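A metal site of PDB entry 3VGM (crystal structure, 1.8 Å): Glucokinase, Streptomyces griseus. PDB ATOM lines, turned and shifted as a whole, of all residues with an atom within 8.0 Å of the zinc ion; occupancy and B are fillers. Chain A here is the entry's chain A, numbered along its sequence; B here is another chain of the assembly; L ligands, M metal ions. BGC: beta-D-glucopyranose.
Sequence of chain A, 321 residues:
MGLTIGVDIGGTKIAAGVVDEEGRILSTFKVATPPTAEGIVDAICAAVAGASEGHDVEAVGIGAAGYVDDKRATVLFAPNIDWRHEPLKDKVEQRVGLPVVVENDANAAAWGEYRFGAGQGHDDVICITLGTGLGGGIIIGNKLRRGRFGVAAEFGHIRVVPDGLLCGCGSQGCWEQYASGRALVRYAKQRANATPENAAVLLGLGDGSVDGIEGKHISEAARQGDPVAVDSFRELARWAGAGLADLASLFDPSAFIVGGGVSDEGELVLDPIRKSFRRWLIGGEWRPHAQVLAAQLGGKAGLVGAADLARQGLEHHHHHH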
ATOM      1  N   TYR A  67     -29.211  -9.502  -4.507  1.00  0.00           N
ATOM      2  CA  TYR A  67     -28.083  -8.589  -4.660  1.00  0.00           C
ATOM      3  C   TYR A  67     -28.367  -7.771  -5.904  1.00  0.00           C
ATOM      4  O   TYR A  67     -28.525  -8.325  -7.002  1.00  0.00           O
ATOM      5  CB  TYR A  67     -26.741  -9.362  -4.791  1.00  0.00           C
ATOM      6  CG  TYR A  67     -26.651 -10.595  -3.940  1.00  0.00           C
ATOM      7  CD1 TYR A  67     -27.103 -10.588  -2.618  1.00  0.00           C
ATOM      8  CD2 TYR A  67     -26.108 -11.783  -4.463  1.00  0.00           C
ATOM      9  CE1 TYR A  67     -27.042 -11.751  -1.832  1.00  0.00           C
ATOM     10  CE2 TYR A  67     -26.036 -12.939  -3.683  1.00  0.00           C
ATOM     11  CZ  TYR A  67     -26.518 -12.914  -2.375  1.00  0.00           C
ATOM     12  OH  TYR A  67     -26.499 -14.055  -1.605  1.00  0.00           O
ATOM     13  N   GLU A 154     -25.729  -6.702   3.117  1.00  0.00           N
ATOM     14  CA  GLU A 154     -26.251  -8.083   3.171  1.00  0.00           C
ATOM     15  C   GLU A 154     -26.058  -8.646   4.595  1.00  0.00           C
ATOM     16  O   GLU A 154     -25.343  -9.639   4.818  1.00  0.00           O
ATOM     17  CB  GLU A 154     -25.594  -8.984   2.113  1.00  0.00           C
ATOM     18  CG  GLU A 154     -26.248  -8.740   0.698  1.00  0.00           C
ATOM     19  CD  GLU A 154     -27.739  -9.130   0.686  1.00  0.00           C
ATOM     20  OE1 GLU A 154     -28.121 -10.121   1.348  1.00  0.00           O
ATOM     21  OE2 GLU A 154     -28.540  -8.458  -0.009  1.00  0.00           O
ATOM     22  N   PHE A 155     -26.699  -7.978   5.553  1.00  0.00           N
ATOM     23  CA  PHE A 155     -26.584  -8.364   6.975  1.00  0.00           C
ATOM     24  C   PHE A 155     -26.987  -9.808   7.255  1.00  0.00           C
ATOM     25  O   PHE A 155     -26.460 -10.424   8.179  1.00  0.00           O
ATOM     26  CB  PHE A 155     -27.485  -7.459   7.831  1.00  0.00           C
ATOM     27  CG  PHE A 155     -27.086  -6.003   7.787  1.00  0.00           C
ATOM     28  CD1 PHE A 155     -25.764  -5.619   7.776  1.00  0.00           C
ATOM     29  CD2 PHE A 155     -28.035  -5.017   7.804  1.00  0.00           C
ATOM     30  CE1 PHE A 155     -25.389  -4.260   7.755  1.00  0.00           C
ATOM     31  CE2 PHE A 155     -27.670  -3.634   7.793  1.00  0.00           C
ATOM     32  CZ  PHE A 155     -26.343  -3.272   7.763  1.00  0.00           C
ATOM     33  N   GLY A 156     -27.942 -10.317   6.488  1.00  0.00           N
ATOM     34  CA  GLY A 156     -28.402 -11.683   6.711  1.00  0.00           C
ATOM     35  C   GLY A 156     -27.309 -12.710   6.506  1.00  0.00           C
ATOM     36  O   GLY A 156     -27.431 -13.814   7.011  1.00  0.00           O
ATOM     37  N   HIS A 157     -26.258 -12.359   5.759  1.00  0.00           N
ATOM     38  CA  HIS A 157     -25.243 -13.345   5.395  1.00  0.00           C
ATOM     39  C   HIS A 157     -23.865 -13.097   5.991  1.00  0.00           C
ATOM     40  O   HIS A 157     -22.861 -13.655   5.515  1.00  0.00           O
ATOM     41  CB  HIS A 157     -25.242 -13.540   3.866  1.00  0.00           C
ATOM     42  CG  HIS A 157     -26.624 -13.828   3.351  1.00  0.00           C
ATOM     43  ND1 HIS A 157     -27.258 -15.032   3.584  1.00  0.00           N
ATOM     44  CD2 HIS A 157     -27.547 -13.028   2.735  1.00  0.00           C
ATOM     45  CE1 HIS A 157     -28.485 -14.999   3.071  1.00  0.00           C
ATOM     46  NE2 HIS A 157     -28.692 -13.784   2.574  1.00  0.00           N
ATOM     47  N   ILE A 158     -23.810 -12.308   7.065  1.00  0.00           N
ATOM     48  CA  ILE A 158     -22.578 -12.309   7.872  1.00  0.00           C
ATOM     49  C   ILE A 158     -22.553 -13.597   8.708  1.00  0.00           C
ATOM     50  O   ILE A 158     -23.592 -14.066   9.183  1.00  0.00           O
ATOM     51  CB  ILE A 158     -22.474 -11.067   8.787  1.00  0.00           C
ATOM     52  CG1 ILE A 158     -23.621 -11.017   9.790  1.00  0.00           C
ATOM     53  CG2 ILE A 158     -22.459  -9.780   7.936  1.00  0.00           C
ATOM     54  CD1 ILE A 158     -23.502  -9.913  10.866  1.00  0.00           C
ATOM     55  N   ARG A 159     -21.359 -14.183   8.878  1.00  0.00           N
ATOM     56  CA  ARG A 159     -21.240 -15.445   9.571  1.00  0.00           C
ATOM     57  C   ARG A 159     -21.233 -15.211  11.077  1.00  0.00           C
ATOM     58  O   ARG A 159     -20.298 -14.665  11.608  1.00  0.00           O
ATOM     59  CB  ARG A 159     -19.954 -16.174   9.169  1.00  0.00           C
ATOM     60  CG  ARG A 159     -19.914 -17.602   9.727  1.00  0.00           C
ATOM     61  CD  ARG A 159     -18.622 -18.342   9.319  1.00  0.00           C
ATOM     62  NE  ARG A 159     -17.492 -17.787  10.049  1.00  0.00           N
ATOM     63  CZ  ARG A 159     -16.246 -18.264   9.986  1.00  0.00           C
ATOM     64  NH1 ARG A 159     -15.971 -19.328   9.250  1.00  0.00           N
ATOM     65  NH2 ARG A 159     -15.295 -17.670  10.696  1.00  0.00           N
ATOM     66  N   LEU A 165     -25.180 -23.496  10.296  1.00  0.00           N
ATOM     67  CA  LEU A 165     -26.214 -23.985   9.392  1.00  0.00           C
ATOM     68  C   LEU A 165     -25.998 -23.586   7.935  1.00  0.00           C
ATOM     69  O   LEU A 165     -25.661 -22.425   7.637  1.00  0.00           O
ATOM     70  CB  LEU A 165     -27.590 -23.450   9.869  1.00  0.00           C
ATOM     71  CG  LEU A 165     -28.107 -24.099  11.142  1.00  0.00           C
ATOM     72  CD1 LEU A 165     -29.285 -23.234  11.679  1.00  0.00           C
ATOM     73  CD2 LEU A 165     -28.646 -25.519  10.801  1.00  0.00           C
ATOM     74  N   LEU A 166     -26.272 -24.522   7.017  1.00  0.00           N
ATOM     75  CA  LEU A 166     -26.272 -24.188   5.582  1.00  0.00           C
ATOM     76  C   LEU A 166     -27.364 -23.164   5.313  1.00  0.00           C
ATOM     77  O   LEU A 166     -28.486 -23.289   5.819  1.00  0.00           O
ATOM     78  CB  LEU A 166     -26.562 -25.440   4.728  1.00  0.00           C
ATOM     79  CG  LEU A 166     -25.527 -26.543   4.755  1.00  0.00           C
ATOM     80  CD1 LEU A 166     -26.087 -27.803   4.091  1.00  0.00           C
ATOM     81  CD2 LEU A 166     -24.227 -26.094   4.090  1.00  0.00           C
ATOM     82  N   CYS A 167     -27.041 -22.158   4.510  1.00  0.00           N
ATOM     83  CA  CYS A 167     -27.947 -21.061   4.191  1.00  0.00           C
ATOM     84  C   CYS A 167     -28.313 -21.073   2.696  1.00  0.00           C
ATOM     85  O   CYS A 167     -27.579 -21.631   1.877  1.00  0.00           O
ATOM     86  CB  CYS A 167     -27.240 -19.749   4.547  1.00  0.00           C
ATOM     87  SG  CYS A 167     -28.226 -18.215   4.297  1.00  0.00           S
ATOM     88  N   GLY A 168     -29.456 -20.481   2.347  1.00  0.00           N
ATOM     89  CA  GLY A 168     -29.864 -20.356   0.953  1.00  0.00           C
ATOM     90  C   GLY A 168     -28.872 -19.596   0.087  1.00  0.00           C
ATOM     91  O   GLY A 168     -28.862 -19.772  -1.153  1.00  0.00           O
ATOM     92  N   CYS A 169     -28.039 -18.743   0.691  1.00  0.00           N
ATOM     93  CA  CYS A 169     -27.009 -18.024  -0.086  1.00  0.00           C
ATOM     94  C   CYS A 169     -25.895 -18.923  -0.610  1.00  0.00           C
ATOM     95  O   CYS A 169     -25.135 -18.504  -1.491  1.00  0.00           O
ATOM     96  CB  CYS A 169     -26.414 -16.866   0.719  1.00  0.00           C
ATOM     97  SG  CYS A 169     -25.240 -17.408   1.990  1.00  0.00           S
ATOM     98  N   GLY A 170     -25.784 -20.133  -0.073  1.00  0.00           N
ATOM     99  CA  GLY A 170     -24.720 -21.059  -0.446  1.00  0.00           C
ATOM    100  C   GLY A 170     -23.647 -21.233   0.630  1.00  0.00           C
ATOM    101  O   GLY A 170     -22.814 -22.126   0.537  1.00  0.00           O
ATOM    102  N   SER A 171     -23.649 -20.366   1.647  1.00  0.00           N
ATOM    103  CA  SER A 171     -22.619 -20.404   2.679  1.00  0.00           C
ATOM    104  C   SER A 171     -23.142 -21.104   3.947  1.00  0.00           C
ATOM    105  O   SER A 171     -24.173 -21.797   3.903  1.00  0.00           O
ATOM    106  CB  SER A 171     -22.124 -18.983   3.013  1.00  0.00           C
ATOM    107  OG  SER A 171     -20.859 -19.056   3.664  1.00  0.00           O
ATOM    108  N   GLN A 172     -22.416 -20.913   5.064  1.00  0.00           N
ATOM    109  CA  GLN A 172     -22.758 -21.507   6.352  1.00  0.00           C
ATOM    110  C   GLN A 172     -22.735 -20.481   7.465  1.00  0.00           C
ATOM    111  O   GLN A 172     -21.858 -19.601   7.486  1.00  0.00           O
ATOM    112  CB  GLN A 172     -21.711 -22.538   6.772  1.00  0.00           C
ATOM    113  CG  GLN A 172     -21.956 -23.916   6.206  1.00  0.00           C
ATOM    114  CD  GLN A 172     -20.879 -24.882   6.678  1.00  0.00           C
ATOM    115  OE1 GLN A 172     -19.971 -25.208   5.907  1.00  0.00           O
ATOM    116  NE2 GLN A 172     -20.962 -25.350   7.926  1.00  0.00           N
ATOM    117  N   GLY A 173     -23.633 -20.675   8.418  1.00  0.00           N
ATOM    118  CA  GLY A 173     -23.550 -19.954   9.716  1.00  0.00           C
ATOM    119  C   GLY A 173     -24.047 -18.533   9.667  1.00  0.00           C
ATOM    120  O   GLY A 173     -23.765 -17.755  10.588  1.00  0.00           O
ATOM    121  N   CYS A 174     -24.768 -18.185   8.594  1.00  0.00           N
ATOM    122  CA  CYS A 174     -25.313 -16.824   8.396  1.00  0.00           C
ATOM    123  C   CYS A 174     -26.299 -16.371   9.484  1.00  0.00           C
ATOM    124  O   CYS A 174     -27.122 -17.148   9.992  1.00  0.00           O
ATOM    125  CB  CYS A 174     -26.046 -16.776   7.034  1.00  0.00           C
ATOM    126  SG  CYS A 174     -24.893 -17.099   5.687  1.00  0.00           S
ATOM    127  N   TRP A 175     -26.247 -15.067   9.790  1.00  0.00           N
ATOM    128  CA  TRP A 175     -27.133 -14.466  10.802  1.00  0.00           C
ATOM    129  C   TRP A 175     -28.607 -14.799  10.510  1.00  0.00           C
ATOM    130  O   TRP A 175     -29.380 -15.059  11.416  1.00  0.00           O
ATOM    131  CB  TRP A 175     -26.918 -12.959  10.816  1.00  0.00           C
ATOM    132  CG  TRP A 175     -27.473 -12.240  12.017  1.00  0.00           C
ATOM    133  CD1 TRP A 175     -27.805 -12.764  13.238  1.00  0.00           C
ATOM    134  CD2 TRP A 175     -27.717 -10.835  12.100  1.00  0.00           C
ATOM    135  NE1 TRP A 175     -28.275 -11.770  14.079  1.00  0.00           N
ATOM    136  CE2 TRP A 175     -28.234 -10.572  13.389  1.00  0.00           C
ATOM    137  CE3 TRP A 175     -27.534  -9.760  11.197  1.00  0.00           C
ATOM    138  CZ2 TRP A 175     -28.570  -9.295  13.815  1.00  0.00           C
ATOM    139  CZ3 TRP A 175     -27.902  -8.475  11.609  1.00  0.00           C
ATOM    140  CH2 TRP A 175     -28.384  -8.252  12.928  1.00  0.00           C
ATOM    141  N   GLU A 176     -28.967 -14.832   9.226  1.00  0.00           N
ATOM    142  CA  GLU A 176     -30.328 -15.146   8.801  1.00  0.00           C
ATOM    143  C   GLU A 176     -30.793 -16.530   9.254  1.00  0.00           C
ATOM    144  O   GLU A 176     -31.975 -16.733   9.495  1.00  0.00           O
ATOM    145  CB  GLU A 176     -30.388 -15.055   7.254  1.00  0.00           C
ATOM    146  CG  GLU A 176     -31.661 -15.570   6.626  1.00  0.00           C
ATOM    147  CD  GLU A 176     -31.723 -15.199   5.143  1.00  0.00           C
ATOM    148  OE1 GLU A 176     -31.838 -13.987   4.863  1.00  0.00           O
ATOM    149  OE2 GLU A 176     -31.606 -16.096   4.299  1.00  0.00           O
ATOM    150  N   GLN A 177     -29.857 -17.480   9.434  1.00  0.00           N
ATOM    151  CA  GLN A 177     -30.214 -18.811   9.911  1.00  0.00           C
ATOM    152  C   GLN A 177     -30.564 -18.831  11.403  1.00  0.00           C
ATOM    153  O   GLN A 177     -31.099 -19.832  11.873  1.00  0.00           O
ATOM    154  CB  GLN A 177     -29.077 -19.819   9.655  1.00  0.00           C
ATOM    155  CG  GLN A 177     -28.897 -20.115   8.135  1.00  0.00           C
ATOM    156  CD  GLN A 177     -30.214 -20.494   7.463  1.00  0.00           C
ATOM    157  OE1 GLN A 177     -30.914 -21.388   7.942  1.00  0.00           O
ATOM    158  NE2 GLN A 177     -30.549 -19.817   6.325  1.00  0.00           N
ATOM    159  N   SER B 249     -19.783  -8.447   2.857  1.00  0.00           N
ATOM    160  CA  SER B 249     -21.260  -8.457   2.928  1.00  0.00           C
ATOM    161  C   SER B 249     -21.820  -7.221   3.604  1.00  0.00           C
ATOM    162  O   SER B 249     -22.941  -6.802   3.283  1.00  0.00           O
ATOM    163  CB  SER B 249     -21.753  -9.697   3.656  1.00  0.00           C
ATOM    164  OG  SER B 249     -21.623 -10.764   2.737  1.00  0.00           O
ATOM    165  N   ILE B 282     -19.977 -14.443   0.335  1.00  0.00           N
ATOM    166  CA  ILE B 282     -21.334 -14.944   0.008  1.00  0.00           C
ATOM    167  C   ILE B 282     -21.747 -14.361  -1.326  1.00  0.00           C
ATOM    168  O   ILE B 282     -21.472 -13.184  -1.628  1.00  0.00           O
ATOM    169  CB  ILE B 282     -22.369 -14.695   1.142  1.00  0.00           C
ATOM    170  CG1 ILE B 282     -22.670 -13.202   1.303  1.00  0.00           C
ATOM    171  CG2 ILE B 282     -21.902 -15.303   2.508  1.00  0.00           C
ATOM    172  CD1 ILE B 282     -24.001 -12.789   0.550  1.00  0.00           C
ATOM    173  N   GLY B 283     -22.381 -15.188  -2.155  1.00  0.00           N
ATOM    174  CA  GLY B 283     -22.791 -14.751  -3.481  1.00  0.00           C
ATOM    175  C   GLY B 283     -21.625 -14.495  -4.418  1.00  0.00           C
ATOM    176  O   GLY B 283     -21.772 -13.807  -5.437  1.00  0.00           O
HETATM  177  C2  BGC L   1     -31.301 -11.480   0.954  1.00  0.00           C
HETATM  178  C3  BGC L   1     -31.388  -9.953   1.015  1.00  0.00           C
HETATM  179  C4  BGC L   1     -32.786  -9.474   1.411  1.00  0.00           C
HETATM  180  C5  BGC L   1     -33.304 -10.238   2.641  1.00  0.00           C
HETATM  181  C6  BGC L   1     -34.748  -9.850   2.991  1.00  0.00           C
HETATM  182  C1  BGC L   1     -31.861 -12.025   2.287  1.00  0.00           C
HETATM  183  O1  BGC L   1     -31.833 -13.411   2.302  1.00  0.00           O
HETATM  184  O2  BGC L   1     -29.959 -11.912   0.761  1.00  0.00           O
HETATM  185  O3  BGC L   1     -30.976  -9.378  -0.202  1.00  0.00           O
HETATM  186  O4  BGC L   1     -32.748  -8.073   1.694  1.00  0.00           O
HETATM  187  O5  BGC L   1     -33.235 -11.648   2.369  1.00  0.00           O
HETATM  188  O6  BGC L   1     -35.588 -10.175   1.889  1.00  0.00           O
HETATM  189 ZN    ZN M   1     -26.389 -16.854   3.958  1.00  0.00          ZN
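The nearest printed residue that does not touch the zinc ion is Gly 156 (4.4 Å).
The zinc ion is bound by a ring nitrogen (ND1) of His 157, the side-chain sulfur of Cys 174, the side-chain sulfur of Cys 167 and the side-chain sulfur of Cys 169.
The side-chain sulfur (SG) of Cys 169 sits close to the backbone NH (N) of Ser 171 (3.4 Å).
NE2 of Gln 177 sits close to SG of Cys 167 (3.5 Å).
O2 of the ligand lies within hydrogen-bond range of NE2 of His 157.
The side-chain carboxylate of Glu 176 is in hydrogen-bond range of an oxygen (O1) of the ligand (2.6 Å).
The side-chain carboxylate (OE2) of Glu 154 lies within hydrogen-bond range of an oxygen (O3) of the ligand.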
